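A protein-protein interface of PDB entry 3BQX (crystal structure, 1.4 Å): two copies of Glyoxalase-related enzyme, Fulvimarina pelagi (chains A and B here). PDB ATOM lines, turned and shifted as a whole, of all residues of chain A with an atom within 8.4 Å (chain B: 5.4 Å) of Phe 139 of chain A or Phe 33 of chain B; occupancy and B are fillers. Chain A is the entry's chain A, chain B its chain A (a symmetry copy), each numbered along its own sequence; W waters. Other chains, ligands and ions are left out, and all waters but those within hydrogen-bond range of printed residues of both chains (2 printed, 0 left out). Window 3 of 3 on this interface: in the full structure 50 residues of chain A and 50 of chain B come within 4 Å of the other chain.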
ATOM      1  N   ASN A 126      26.985 -30.698  -5.871  1.00  0.00           N
ATOM      2  CA  ASN A 126      27.843 -29.544  -5.623  1.00  0.00           C
ATOM      3  C   ASN A 126      27.811 -29.306  -4.118  1.00  0.00           C
ATOM      4  O   ASN A 126      26.954 -28.583  -3.608  1.00  0.00           O
ATOM      5  CB  ASN A 126      27.316 -28.306  -6.350  1.00  0.00           C
ATOM      6  CG  ASN A 126      28.295 -27.150  -6.302  1.00  0.00           C
ATOM      7  OD1 ASN A 126      28.996 -26.961  -5.308  1.00  0.00           O
ATOM      8  ND2 ASN A 126      28.341 -26.365  -7.372  1.00  0.00           N
ATOM      9  N   VAL A 128      29.515 -27.450  -2.223  1.00  0.00           N
ATOM     10  CA  VAL A 128      29.781 -26.092  -1.773  1.00  0.00           C
ATOM     11  C   VAL A 128      28.512 -25.293  -1.480  1.00  0.00           C
ATOM     12  O   VAL A 128      28.514 -24.420  -0.612  1.00  0.00           O
ATOM     13  CB  VAL A 128      30.640 -25.331  -2.809  1.00  0.00           C
ATOM     14  CG1 VAL A 128      30.960 -23.938  -2.301  1.00  0.00           C
ATOM     15  CG2 VAL A 128      31.927 -26.104  -3.079  1.00  0.00           C
ATOM     16  N   TRP A 129      27.431 -25.595  -2.195  1.00  0.00           N
ATOM     17  CA  TRP A 129      26.158 -24.894  -2.002  1.00  0.00           C
ATOM     18  C   TRP A 129      25.231 -25.667  -1.062  1.00  0.00           C
ATOM     19  O   TRP A 129      24.777 -26.768  -1.377  1.00  0.00           O
ATOM     20  CB  TRP A 129      25.450 -24.698  -3.344  1.00  0.00           C
ATOM     21  CG  TRP A 129      26.173 -23.825  -4.324  1.00  0.00           C
ATOM     22  CD1 TRP A 129      27.485 -23.440  -4.282  1.00  0.00           C
ATOM     23  CD2 TRP A 129      25.635 -23.287  -5.536  1.00  0.00           C
ATOM     24  NE1 TRP A 129      27.796 -22.698  -5.401  1.00  0.00           N
ATOM     25  CE2 TRP A 129      26.679 -22.591  -6.186  1.00  0.00           C
ATOM     26  CE3 TRP A 129      24.369 -23.325  -6.138  1.00  0.00           C
ATOM     27  CZ2 TRP A 129      26.495 -21.940  -7.410  1.00  0.00           C
ATOM     28  CZ3 TRP A 129      24.187 -22.675  -7.356  1.00  0.00           C
ATOM     29  CH2 TRP A 129      25.247 -21.993  -7.977  1.00  0.00           C
ATOM     30  N   PRO A 130      24.929 -25.090   0.107  1.00  0.00           N
ATOM     31  CA  PRO A 130      24.051 -25.741   1.086  1.00  0.00           C
ATOM     32  C   PRO A 130      22.633 -26.016   0.581  1.00  0.00           C
ATOM     33  O   PRO A 130      22.040 -25.195  -0.125  1.00  0.00           O
ATOM     34  CB  PRO A 130      24.054 -24.757   2.256  1.00  0.00           C
ATOM     35  CG  PRO A 130      25.394 -24.104   2.149  1.00  0.00           C
ATOM     36  CD  PRO A 130      25.522 -23.865   0.667  1.00  0.00           C
ATOM     37  N   ILE A 131      22.100 -27.180   0.945  1.00  0.00           N
ATOM     38  CA  ILE A 131      20.742 -27.570   0.586  1.00  0.00           C
ATOM     39  C   ILE A 131      19.994 -27.708   1.912  1.00  0.00           C
ATOM     40  O   ILE A 131      20.306 -28.587   2.719  1.00  0.00           O
ATOM     41  CB  ILE A 131      20.703 -28.927  -0.153  1.00  0.00           C
ATOM     42  CG1 ILE A 131      21.558 -28.868  -1.422  1.00  0.00           C
ATOM     43  CG2 ILE A 131      19.267 -29.286  -0.504  1.00  0.00           C
ATOM     44  CD1 ILE A 131      21.596 -30.181  -2.201  1.00  0.00           C
ATOM     45  N   SER A 136      15.533 -25.501  -0.586  1.00  0.00           N
ATOM     46  CA  SER A 136      16.236 -24.230  -0.443  1.00  0.00           C
ATOM     47  C   SER A 136      17.742 -24.338  -0.652  1.00  0.00           C
ATOM     48  O   SER A 136      18.491 -24.700   0.260  1.00  0.00           O
ATOM     49  CB  SER A 136      15.960 -23.612   0.931  1.00  0.00           C
ATOM     50  OG  SER A 136      16.516 -24.406   1.967  1.00  0.00           O
ATOM     51  N   VAL A 137      18.173 -24.025  -1.868  1.00  0.00           N
ATOM     52  CA  VAL A 137      19.583 -24.055  -2.225  1.00  0.00           C
ATOM     53  C   VAL A 137      20.127 -22.630  -2.166  1.00  0.00           C
ATOM     54  O   VAL A 137      19.504 -21.688  -2.671  1.00  0.00           O
ATOM     55  CB  VAL A 137      19.785 -24.627  -3.650  1.00  0.00           C
ATOM     56  CG1 VAL A 137      21.243 -24.525  -4.060  1.00  0.00           C
ATOM     57  CG2 VAL A 137      19.310 -26.077  -3.694  1.00  0.00           C
ATOM     58  N   THR A 138      21.285 -22.463  -1.540  1.00  0.00           N
ATOM     59  CA  THR A 138      21.876 -21.142  -1.436  1.00  0.00           C
ATOM     60  C   THR A 138      23.306 -21.135  -1.950  1.00  0.00           C
ATOM     61  O   THR A 138      24.092 -22.040  -1.657  1.00  0.00           O
ATOM     62  CB  THR A 138      21.869 -20.641   0.021  1.00  0.00           C
ATOM     63  OG1 THR A 138      22.517 -21.602   0.858  1.00  0.00           O
ATOM     64  CG2 THR A 138      20.445 -20.444   0.509  1.00  0.00           C
ATOM     65  N   PHE A 139      23.630 -20.120  -2.739  1.00  0.00           N
ATOM     66  CA  PHE A 139      24.974 -19.984  -3.270  1.00  0.00           C
ATOM     67  C   PHE A 139      25.938 -19.732  -2.118  1.00  0.00           C
ATOM     68  O   PHE A 139      25.610 -19.030  -1.162  1.00  0.00           O
ATOM     69  CB  PHE A 139      25.063 -18.801  -4.234  1.00  0.00           C
ATOM     70  CG  PHE A 139      26.466 -18.495  -4.678  1.00  0.00           C
ATOM     71  CD1 PHE A 139      27.012 -19.132  -5.784  1.00  0.00           C
ATOM     72  CD2 PHE A 139      27.265 -17.610  -3.952  1.00  0.00           C
ATOM     73  CE1 PHE A 139      28.330 -18.897  -6.165  1.00  0.00           C
ATOM     74  CE2 PHE A 139      28.590 -17.372  -4.331  1.00  0.00           C
ATOM     75  CZ  PHE A 139      29.116 -18.019  -5.437  1.00  0.00           C
ATOM     76  N   ALA A 140      27.129 -20.308  -2.224  1.00  0.00           N
ATOM     77  CA  ALA A 140      28.182 -20.136  -1.229  1.00  0.00           C
ATOM     78  C   ALA A 140      29.496 -20.170  -1.999  1.00  0.00           C
ATOM     79  O   ALA A 140      29.632 -20.922  -2.963  1.00  0.00           O
ATOM     80  CB  ALA A 140      28.138 -21.259  -0.198  1.00  0.00           C
ATOM     81  N   ALA A 141      30.459 -19.354  -1.578  1.00  0.00           N
ATOM     82  CA  ALA A 141      31.753 -19.291  -2.249  1.00  0.00           C
ATOM     83  C   ALA A 141      32.660 -20.450  -1.855  1.00  0.00           C
ATOM     84  O   ALA A 141      32.414 -21.067  -0.796  1.00  0.00           O
ATOM     85  CB  ALA A 141      32.436 -17.965  -1.933  1.00  0.00           C
ATOM     86  N   PRO B  31      23.371  -9.128  -7.893  1.00  0.00           N
ATOM     87  CA  PRO B  31      24.054 -10.419  -7.983  1.00  0.00           C
ATOM     88  C   PRO B  31      24.750 -10.812  -6.689  1.00  0.00           C
ATOM     89  O   PRO B  31      25.126  -9.951  -5.888  1.00  0.00           O
ATOM     90  CB  PRO B  31      25.068 -10.198  -9.107  1.00  0.00           C
ATOM     91  CG  PRO B  31      24.452  -9.107  -9.937  1.00  0.00           C
ATOM     92  CD  PRO B  31      23.909  -8.180  -8.884  1.00  0.00           C
ATOM     93  N   VAL B  32      24.905 -12.118  -6.485  1.00  0.00           N
ATOM     94  CA  VAL B  32      25.628 -12.641  -5.332  1.00  0.00           C
ATOM     95  C   VAL B  32      27.004 -13.069  -5.875  1.00  0.00           C
ATOM     96  O   VAL B  32      27.984 -13.153  -5.135  1.00  0.00           O
ATOM     97  CB  VAL B  32      24.893 -13.847  -4.680  1.00  0.00           C
ATOM     98  CG1 VAL B  32      24.771 -14.996  -5.665  1.00  0.00           C
ATOM     99  CG2 VAL B  32      25.631 -14.299  -3.438  1.00  0.00           C
ATOM    100  N   PHE B  33      27.065 -13.320  -7.182  1.00  0.00           N
ATOM    101  CA  PHE B  33      28.303 -13.701  -7.850  1.00  0.00           C
ATOM    102  C   PHE B  33      28.332 -13.185  -9.282  1.00  0.00           C
ATOM    103  O   PHE B  33      27.307 -13.143  -9.964  1.00  0.00           O
ATOM    104  CB  PHE B  33      28.473 -15.225  -7.898  1.00  0.00           C
ATOM    105  CG  PHE B  33      29.735 -15.665  -8.599  1.00  0.00           C
ATOM    106  CD1 PHE B  33      30.922 -15.831  -7.888  1.00  0.00           C
ATOM    107  CD2 PHE B  33      29.752 -15.858  -9.980  1.00  0.00           C
ATOM    108  CE1 PHE B  33      32.110 -16.179  -8.545  1.00  0.00           C
ATOM    109  CE2 PHE B  33      30.930 -16.204 -10.645  1.00  0.00           C
ATOM    110  CZ  PHE B  33      32.114 -16.364  -9.925  1.00  0.00           C
ATOM    111  N   ARG B  34      29.515 -12.788  -9.736  1.00  0.00           N
ATOM    112  CA  ARG B  34      29.674 -12.327 -11.098  1.00  0.00           C
ATOM    113  C   ARG B  34      31.103 -12.404 -11.588  1.00  0.00           C
ATOM    114  O   ARG B  34      32.035 -12.078 -10.860  1.00  0.00           O
ATOM    115  CB  ARG B  34      29.192 -10.885 -11.256  1.00  0.00           C
ATOM    116  CG  ARG B  34      29.544 -10.303 -12.616  1.00  0.00           C
ATOM    117  CD  ARG B  34      28.937  -8.936 -12.846  1.00  0.00           C
ATOM    118  NE  ARG B  34      29.273  -8.449 -14.182  1.00  0.00           N
ATOM    119  CZ  ARG B  34      28.777  -7.341 -14.722  1.00  0.00           C
ATOM    120  NH1 ARG B  34      27.917  -6.597 -14.042  1.00  0.00           N
ATOM    121  NH2 ARG B  34      29.142  -6.980 -15.946  1.00  0.00           N
ATOM    122  N   ASN B  35      31.267 -12.867 -12.821  1.00  0.00           N
ATOM    123  CA  ASN B  35      32.571 -12.907 -13.461  1.00  0.00           C
ATOM    124  C   ASN B  35      32.289 -12.645 -14.942  1.00  0.00           C
ATOM    125  O   ASN B  35      31.132 -12.498 -15.332  1.00  0.00           O
ATOM    126  CB  ASN B  35      33.318 -14.231 -13.205  1.00  0.00           C
ATOM    127  CG  ASN B  35      32.678 -15.425 -13.871  1.00  0.00           C
ATOM    128  OD1 ASN B  35      31.944 -15.297 -14.843  1.00  0.00           O
ATOM    129  ND2 ASN B  35      32.985 -16.611 -13.358  1.00  0.00           N
ATOM    130  N   ILE B  38      29.460 -15.383 -16.240  1.00  0.00           N
ATOM    131  CA  ILE B  38      28.225 -15.764 -15.565  1.00  0.00           C
ATOM    132  C   ILE B  38      27.861 -14.848 -14.405  1.00  0.00           C
ATOM    133  O   ILE B  38      28.732 -14.227 -13.789  1.00  0.00           O
ATOM    134  CB  ILE B  38      28.346 -17.225 -15.042  1.00  0.00           C
ATOM    135  CG1 ILE B  38      26.973 -17.808 -14.701  1.00  0.00           C
ATOM    136  CG2 ILE B  38      29.253 -17.269 -13.822  1.00  0.00           C
ATOM    137  CD1 ILE B  38      27.004 -19.336 -14.487  1.00  0.00           C
ATOM    138  N   ILE B  39      26.567 -14.760 -14.125  1.00  0.00           N
ATOM    139  CA  ILE B  39      26.062 -13.977 -13.007  1.00  0.00           C
ATOM    140  C   ILE B  39      25.057 -14.839 -12.253  1.00  0.00           C
ATOM    141  O   ILE B  39      24.223 -15.506 -12.870  1.00  0.00           O
ATOM    142  CB  ILE B  39      25.352 -12.684 -13.465  1.00  0.00           C
ATOM    143  CG1 ILE B  39      26.355 -11.767 -14.169  1.00  0.00           C
ATOM    144  CG2 ILE B  39      24.730 -11.979 -12.264  1.00  0.00           C
ATOM    145  CD1 ILE B  39      25.744 -10.501 -14.737  1.00  0.00           C
ATOM    146  N   PHE B  40      25.163 -14.848 -10.927  1.00  0.00           N
ATOM    147  CA  PHE B  40      24.238 -15.599 -10.083  1.00  0.00           C
ATOM    148  C   PHE B  40      23.465 -14.638  -9.195  1.00  0.00           C
ATOM    149  O   PHE B  40      24.044 -13.702  -8.630  1.00  0.00           O
ATOM    150  CB  PHE B  40      24.963 -16.568  -9.135  1.00  0.00           C
ATOM    151  CG  PHE B  40      25.630 -17.736  -9.811  1.00  0.00           C
ATOM    152  CD1 PHE B  40      24.968 -18.491 -10.766  1.00  0.00           C
ATOM    153  CD2 PHE B  40      26.913 -18.116  -9.437  1.00  0.00           C
ATOM    154  CE1 PHE B  40      25.574 -19.613 -11.340  1.00  0.00           C
ATOM    155  CE2 PHE B  40      27.525 -19.235 -10.007  1.00  0.00           C
ATOM    156  CZ  PHE B  40      26.851 -19.981 -10.958  1.00  0.00           C
ATOM    157  N   GLN B  42      20.710 -14.730  -5.919  1.00  0.00           N
ATOM    158  CA  GLN B  42      20.093 -15.606  -4.932  1.00  0.00           C
ATOM    159  C   GLN B  42      18.594 -15.342  -4.923  1.00  0.00           C
ATOM    160  O   GLN B  42      18.156 -14.216  -4.671  1.00  0.00           O
ATOM    161  CB  GLN B  42      20.664 -15.354  -3.535  1.00  0.00           C
ATOM    162  CG  GLN B  42      20.046 -16.271  -2.475  1.00  0.00           C
ATOM    163  CD  GLN B  42      20.358 -17.738  -2.717  1.00  0.00           C
ATOM    164  OE1 GLN B  42      21.518 -18.136  -2.718  1.00  0.00           O
ATOM    165  NE2 GLN B  42      19.322 -18.545  -2.935  1.00  0.00           N
ATOM    166  N   VAL B  47      18.859 -20.532  -7.084  1.00  0.00           N
ATOM    167  CA  VAL B  47      19.708 -19.521  -7.695  1.00  0.00           C
ATOM    168  C   VAL B  47      19.348 -19.338  -9.166  1.00  0.00           C
ATOM    169  O   VAL B  47      19.071 -20.317  -9.865  1.00  0.00           O
ATOM    170  CB  VAL B  47      21.190 -19.948  -7.604  1.00  0.00           C
ATOM    171  CG1 VAL B  47      22.092 -18.911  -8.241  1.00  0.00           C
ATOM    172  CG2 VAL B  47      21.571 -20.161  -6.152  1.00  0.00           C
HETATM  173  O   HOH W   1      23.605 -16.832  -1.586  1.00  0.00           O
HETATM  174  O   HOH W   2      17.464 -20.358  -1.160  1.00  0.00           O
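The side-chain amide nitrogen (NE2) of Gln 42 of chain B is in hydrogen-bond range of the backbone carbonyl oxygen (O) of Val 137 of chain A, 3.2 Å away.
N of Phe 139 of chain A is in hydrogen-bond range of OE1 of Gln 42 of chain B (2.9 Å).
Water W1 bridges OE1 of Gln 42 of chain B (2.7 Å) and O of Phe 139 of chain A (3.0 Å).
Water W2 lies within hydrogen-bond range of O of Val 137 of chain A (2.9 Å) and NE2 of Gln 42 of chain B (3.1 Å).
Printed residues of chain B within 4 Å of Thr 138 of chain A: Gln 42.
Printed residues of chain B within 4 Å of Phe 139 of chain A: Val 32 (3.7 Å), Phe 33 (3.7 Å), Phe 40 (3.7 Å), Gln 42 (2.9 Å) and Val 47 (3.99 Å).
Of chain A, only Phe 139 (3.7 Å) comes within 4 Å of Phe 33 of chain B.
Of the printed residues of chain A, Gln 42 of chain B touches Val 137 (3.2 Å), Thr 138 (3.3 Å) and Phe 139 (2.9 Å).
The nearest residue of chain A that does not touch Phe 33 of chain B is Ala 141 of chain A (6.5 Å).
The nearest printed residue of chain A that does not touch Phe 40 of chain B is Asn 126 of chain A (7.5 Å).
Among the printed residues, no Asp or Glu carboxylate lies within 4 Å of a Lys or Arg side-chain nitrogen of the other chain.
CE2 of Phe 40 of chain B touches CZ2 of Trp 129 of chain A, at 3.9 Å.
Trp 129 of chain A touches Val 47 of chain B.
Thr 138 of chain A touches Gln 42 of chain B.
CD2 of Phe 139 of chain A touches CG2 of Val 32 of chain B (3.7 Å).
Phe 139 of chain A touches Phe 33 of chain B.
Phe 139 of chain A touches Phe 40 of chain B.
Phe 139 of chain A touches Val 47 of chain B.
The backbone NH (N) of Thr 138 of chain A sits at hydrogen-bond distance from the backbone carbonyl oxygen (O) of Pro 130 of chain A (3.2 Å).
The backbone NH of Val 32 of chain B lies within hydrogen-bond range of the backbone carbonyl oxygen of Phe 40 of chain B (2.8 Å).
The backbone NH of Phe 40 of chain B sits at hydrogen-bond distance from the backbone carbonyl oxygen of Phe 33 of chain B, at 2.9 Å.
No position is printed for both chains.
Of the 9 pairs that touch across the chains among the printed residues, none has its exchanged pair printed and touching as well.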
